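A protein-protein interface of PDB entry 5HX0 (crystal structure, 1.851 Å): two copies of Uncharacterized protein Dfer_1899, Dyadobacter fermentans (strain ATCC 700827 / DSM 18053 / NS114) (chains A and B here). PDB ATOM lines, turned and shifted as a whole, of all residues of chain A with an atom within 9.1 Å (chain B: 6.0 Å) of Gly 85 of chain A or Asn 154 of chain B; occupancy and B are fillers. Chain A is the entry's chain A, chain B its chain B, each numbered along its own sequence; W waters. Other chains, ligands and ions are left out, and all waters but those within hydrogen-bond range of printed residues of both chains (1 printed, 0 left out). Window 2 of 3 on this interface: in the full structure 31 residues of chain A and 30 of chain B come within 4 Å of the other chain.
Printed residues of chain B within 4 Å of Gly 85 of chain A: Asn 154 (3.3 Å). Asn 154 of chain B touches one residue of chain A. Printed residues of chain B within 4 Å of Phe 84 of chain A: Gly 151 and Ala 199. Printed residues of chain B within 4 Å of Lys 87 of chain A: Asp 150 (2.8 Å). Val 83 of chain A touches none of the printed residues of chain B. The nearest residue of chain B that does not touch Gly 85 of chain A is Asp 150 of chain B (4.1 Å).
Water W1 lies within hydrogen-bond range of O of Gly 151 of chain B (2.6 Å), O of Phe 84 of chain A (2.8 Å) and N of Leu 155 of chain B (3.4 Å).
The side-chain carboxylate of Glu 86 of chain A lies within salt-bridge range of the guanidinium group of Arg 81 of chain A (2.9 Å). O of Asp 150 of chain B sits at hydrogen-bond distance from ND2 of Asn 154 of chain B (3.1 Å).
No position is printed for both chains.
Among the printed residues, pairs that only touch across the chains: Phe 84 of chain A with Gly 151 of chain B (3.5 Å), Glu 86 of chain A with Asp 150 of chain B (3.5 Å), Glu 86 of chain A with Gly 151 of chain B (3.6 Å) and Phe 84 of chain A with Ala 199 of chain B (3.7 Å).
The side-chain amide nitrogen of Asn 154 of chain B is in hydrogen-bond range of the backbone carbonyl oxygen of Gly 85 of chain A, 3.3 Å away. N of Lys 87 of chain A is in hydrogen-bond range of OD2 of Asp 150 of chain B (2.8 Å).
Of the 9 printed residues of chain A, 4 touch a printed residue of chain B. Hydrophobic or aromatic side chains of chain A that line the printed part of chain B: Phe 84.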
ATOM      1  N   ASP A  80      13.066 -12.780 -24.799  1.00  0.00           N
ATOM      2  CA  ASP A  80      13.724 -13.876 -24.094  1.00  0.00           C
ATOM      3  C   ASP A  80      12.784 -14.304 -22.980  1.00  0.00           C
ATOM      4  O   ASP A  80      12.474 -13.497 -22.101  1.00  0.00           O
ATOM      5  CB  ASP A  80      15.072 -13.447 -23.522  1.00  0.00           C
ATOM      6  CG  ASP A  80      15.861 -14.634 -22.943  1.00  0.00           C
ATOM      7  OD1 ASP A  80      15.303 -15.395 -22.107  1.00  0.00           O
ATOM      8  OD2 ASP A  80      17.030 -14.829 -23.356  1.00  0.00           O
ATOM      9  N   ARG A  81      12.309 -15.557 -23.031  1.00  0.00           N
ATOM     10  CA  ARG A  81      11.235 -15.977 -22.135  1.00  0.00           C
ATOM     11  C   ARG A  81      11.664 -15.963 -20.677  1.00  0.00           C
ATOM     12  O   ARG A  81      10.803 -16.055 -19.793  1.00  0.00           O
ATOM     13  CB  ARG A  81      10.720 -17.371 -22.533  1.00  0.00           C
ATOM     14  CG  ARG A  81      10.214 -17.463 -24.010  1.00  0.00           C
ATOM     15  CD  ARG A  81       9.048 -16.533 -24.270  1.00  0.00           C
ATOM     16  NE  ARG A  81       7.882 -16.938 -23.477  1.00  0.00           N
ATOM     17  CZ  ARG A  81       6.628 -16.554 -23.728  1.00  0.00           C
ATOM     18  NH1 ARG A  81       6.357 -15.745 -24.745  1.00  0.00           N
ATOM     19  NH2 ARG A  81       5.639 -16.971 -22.949  1.00  0.00           N
ATOM     20  N   LYS A  82      12.972 -15.829 -20.398  1.00  0.00           N
ATOM     21  CA  LYS A  82      13.397 -15.647 -19.014  1.00  0.00           C
ATOM     22  C   LYS A  82      12.806 -14.392 -18.381  1.00  0.00           C
ATOM     23  O   LYS A  82      12.673 -14.342 -17.152  1.00  0.00           O
ATOM     24  CB  LYS A  82      14.925 -15.614 -18.926  1.00  0.00           C
ATOM     25  CG  LYS A  82      15.543 -17.004 -19.057  1.00  0.00           C
ATOM     26  CD  LYS A  82      17.060 -16.933 -19.198  1.00  0.00           C
ATOM     27  CE  LYS A  82      17.672 -18.312 -19.392  1.00  0.00           C
ATOM     28  NZ  LYS A  82      19.093 -18.216 -19.852  1.00  0.00           N
ATOM     29  N   VAL A  83      12.417 -13.387 -19.173  1.00  0.00           N
ATOM     30  CA  VAL A  83      11.760 -12.223 -18.564  1.00  0.00           C
ATOM     31  C   VAL A  83      10.414 -12.587 -17.928  1.00  0.00           C
ATOM     32  O   VAL A  83       9.898 -11.835 -17.092  1.00  0.00           O
ATOM     33  CB  VAL A  83      11.543 -11.061 -19.557  1.00  0.00           C
ATOM     34  CG1 VAL A  83      12.862 -10.613 -20.213  1.00  0.00           C
ATOM     35  CG2 VAL A  83      10.413 -11.399 -20.593  1.00  0.00           C
ATOM     36  N   PHE A  84       9.811 -13.701 -18.331  1.00  0.00           N
ATOM     37  CA  PHE A  84       8.580 -14.189 -17.722  1.00  0.00           C
ATOM     38  C   PHE A  84       8.828 -15.294 -16.703  1.00  0.00           C
ATOM     39  O   PHE A  84       7.884 -16.007 -16.332  1.00  0.00           O
ATOM     40  CB  PHE A  84       7.630 -14.709 -18.794  1.00  0.00           C
ATOM     41  CG  PHE A  84       7.230 -13.675 -19.808  1.00  0.00           C
ATOM     42  CD1 PHE A  84       6.697 -12.453 -19.408  1.00  0.00           C
ATOM     43  CD2 PHE A  84       7.387 -13.931 -21.166  1.00  0.00           C
ATOM     44  CE1 PHE A  84       6.317 -11.496 -20.352  1.00  0.00           C
ATOM     45  CE2 PHE A  84       7.009 -12.982 -22.110  1.00  0.00           C
ATOM     46  CZ  PHE A  84       6.479 -11.768 -21.701  1.00  0.00           C
ATOM     47  N   GLY A  85      10.073 -15.489 -16.276  1.00  0.00           N
ATOM     48  CA  GLY A  85      10.341 -16.557 -15.325  1.00  0.00           C
ATOM     49  C   GLY A  85      10.305 -17.948 -15.909  1.00  0.00           C
ATOM     50  O   GLY A  85      10.243 -18.923 -15.152  1.00  0.00           O
ATOM     51  N   GLU A  86      10.344 -18.083 -17.235  1.00  0.00           N
ATOM     52  CA  GLU A  86      10.309 -19.406 -17.841  1.00  0.00           C
ATOM     53  C   GLU A  86      11.728 -19.969 -17.970  1.00  0.00           C
ATOM     54  O   GLU A  86      12.721 -19.266 -17.801  1.00  0.00           O
ATOM     55  CB  GLU A  86       9.588 -19.344 -19.194  1.00  0.00           C
ATOM     56  CG  GLU A  86       8.183 -18.731 -19.055  1.00  0.00           C
ATOM     57  CD  GLU A  86       7.426 -18.580 -20.371  1.00  0.00           C
ATOM     58  OE1 GLU A  86       7.950 -18.971 -21.444  1.00  0.00           O
ATOM     59  OE2 GLU A  86       6.288 -18.054 -20.318  1.00  0.00           O
ATOM     60  N   LYS A  87      11.811 -21.268 -18.264  1.00  0.00           N
ATOM     61  CA  LYS A  87      13.094 -21.970 -18.248  1.00  0.00           C
ATOM     62  C   LYS A  87      13.978 -21.635 -19.453  1.00  0.00           C
ATOM     63  O   LYS A  87      15.214 -21.612 -19.323  1.00  0.00           O
ATOM     64  CB  LYS A  87      12.844 -23.482 -18.178  1.00  0.00           C
ATOM     65  CG  LYS A  87      12.042 -24.009 -19.370  1.00  0.00           C
ATOM     66  CD  LYS A  87      11.707 -25.486 -19.253  1.00  0.00           C
ATOM     67  CE  LYS A  87      11.034 -25.976 -20.525  1.00  0.00           C
ATOM     68  NZ  LYS A  87      11.907 -25.719 -21.704  1.00  0.00           N
ATOM     69  N   GLY A  88      13.391 -21.399 -20.622  1.00  0.00           N
ATOM     70  CA  GLY A  88      14.193 -21.125 -21.804  1.00  0.00           C
ATOM     71  C   GLY A  88      13.303 -20.628 -22.926  1.00  0.00           C
ATOM     72  O   GLY A  88      12.083 -20.503 -22.776  1.00  0.00           O
ATOM     73  N   PRO B 149       3.242 -22.526 -18.871  1.00  0.00           N
ATOM     74  CA  PRO B 149       2.945 -23.016 -17.508  1.00  0.00           C
ATOM     75  C   PRO B 149       4.062 -22.802 -16.510  1.00  0.00           C
ATOM     76  O   PRO B 149       3.790 -22.404 -15.367  1.00  0.00           O
ATOM     77  CB  PRO B 149       2.680 -24.507 -17.739  1.00  0.00           C
ATOM     78  CG  PRO B 149       2.075 -24.558 -19.105  1.00  0.00           C
ATOM     79  CD  PRO B 149       2.888 -23.534 -19.893  1.00  0.00           C
ATOM     80  N   ASP B 150       5.319 -23.044 -16.893  1.00  0.00           N
ATOM     81  CA  ASP B 150       6.382 -22.866 -15.911  1.00  0.00           C
ATOM     82  C   ASP B 150       6.535 -21.398 -15.534  1.00  0.00           C
ATOM     83  O   ASP B 150       6.897 -21.084 -14.390  1.00  0.00           O
ATOM     84  CB  ASP B 150       7.710 -23.466 -16.410  1.00  0.00           C
ATOM     85  CG  ASP B 150       8.247 -22.807 -17.691  1.00  0.00           C
ATOM     86  OD1 ASP B 150       7.460 -22.277 -18.498  1.00  0.00           O
ATOM     87  OD2 ASP B 150       9.481 -22.852 -17.905  1.00  0.00           O
ATOM     88  N   GLY B 151       6.236 -20.485 -16.458  1.00  0.00           N
ATOM     89  CA  GLY B 151       6.242 -19.080 -16.098  1.00  0.00           C
ATOM     90  C   GLY B 151       5.119 -18.743 -15.137  1.00  0.00           C
ATOM     91  O   GLY B 151       5.308 -17.977 -14.185  1.00  0.00           O
ATOM     92  N   MET B 152       3.938 -19.301 -15.378  1.00  0.00           N
ATOM     93  CA  MET B 152       2.782 -19.100 -14.503  1.00  0.00           C
ATOM     94  C   MET B 152       3.092 -19.555 -13.078  1.00  0.00           C
ATOM     95  O   MET B 152       2.738 -18.862 -12.124  1.00  0.00           O
ATOM     96  CB  MET B 152       1.553 -19.856 -15.018  1.00  0.00           C
ATOM     97  CG  MET B 152       0.986 -19.370 -16.346  1.00  0.00           C
ATOM     98  SD  MET B 152       0.360 -17.534 -16.241  1.00  0.00           S
ATOM     99  CE  MET B 152      -0.950 -17.714 -14.805  1.00  0.00           C
ATOM    100  N   GLU B 153       3.739 -20.724 -12.950  1.00  0.00           N
ATOM    101  CA  GLU B 153       4.045 -21.269 -11.624  1.00  0.00           C
ATOM    102  C   GLU B 153       4.974 -20.357 -10.829  1.00  0.00           C
ATOM    103  O   GLU B 153       4.895 -20.323  -9.598  1.00  0.00           O
ATOM    104  CB  GLU B 153       4.665 -22.667 -11.752  1.00  0.00           C
ATOM    105  CG  GLU B 153       3.698 -23.708 -12.309  1.00  0.00           C
ATOM    106  CD  GLU B 153       4.352 -25.057 -12.554  1.00  0.00           C
ATOM    107  OE1 GLU B 153       4.554 -25.805 -11.575  1.00  0.00           O
ATOM    108  OE2 GLU B 153       4.669 -25.371 -13.724  1.00  0.00           O
ATOM    109  N   ASN B 154       5.850 -19.609 -11.499  1.00  0.00           N
ATOM    110  CA  ASN B 154       6.853 -18.817 -10.793  1.00  0.00           C
ATOM    111  C   ASN B 154       6.442 -17.365 -10.563  1.00  0.00           C
ATOM    112  O   ASN B 154       7.242 -16.596 -10.027  1.00  0.00           O
ATOM    113  CB  ASN B 154       8.184 -18.853 -11.557  1.00  0.00           C
ATOM    114  CG  ASN B 154       8.892 -20.198 -11.431  1.00  0.00           C
ATOM    115  OD1 ASN B 154       8.960 -20.779 -10.345  1.00  0.00           O
ATOM    116  ND2 ASN B 154       9.413 -20.700 -12.547  1.00  0.00           N
ATOM    117  N   LEU B 155       5.231 -16.971 -10.953  1.00  0.00           N
ATOM    118  CA  LEU B 155       4.843 -15.568 -10.866  1.00  0.00           C
ATOM    119  C   LEU B 155       4.863 -15.047  -9.437  1.00  0.00           C
ATOM    120  O   LEU B 155       4.356 -15.687  -8.522  1.00  0.00           O
ATOM    121  CB  LEU B 155       3.450 -15.380 -11.428  1.00  0.00           C
ATOM    122  CG  LEU B 155       3.390 -15.209 -12.945  1.00  0.00           C
ATOM    123  CD1 LEU B 155       1.938 -15.308 -13.360  1.00  0.00           C
ATOM    124  CD2 LEU B 155       4.011 -13.857 -13.348  1.00  0.00           C
ATOM    125  N   LYS B 156       5.400 -13.843  -9.261  1.00  0.00           N
ATOM    126  CA  LYS B 156       5.267 -13.160  -7.985  1.00  0.00           C
ATOM    127  C   LYS B 156       3.819 -12.714  -7.792  1.00  0.00           C
ATOM    128  O   LYS B 156       3.213 -12.157  -8.710  1.00  0.00           O
ATOM    129  CB  LYS B 156       6.213 -11.960  -7.931  1.00  0.00           C
ATOM    130  CG  LYS B 156       6.287 -11.315  -6.557  1.00  0.00           C
ATOM    131  CD  LYS B 156       7.408 -10.299  -6.478  1.00  0.00           C
ATOM    132  CE  LYS B 156       7.546  -9.736  -5.057  1.00  0.00           C
ATOM    133  NZ  LYS B 156       8.555 -10.441  -4.209  1.00  0.00           N
ATOM    134  N   ALA B 199       3.481  -9.325 -15.257  1.00  0.00           N
ATOM    135  CA  ALA B 199       3.935 -10.636 -15.704  1.00  0.00           C
ATOM    136  C   ALA B 199       5.452 -10.770 -15.687  1.00  0.00           C
ATOM    137  O   ALA B 199       5.961 -11.893 -15.787  1.00  0.00           O
ATOM    138  CB  ALA B 199       3.415 -10.903 -17.120  1.00  0.00           C
HETATM  139  O   HOH W   1       7.141 -16.183 -13.619  1.00  0.00           O
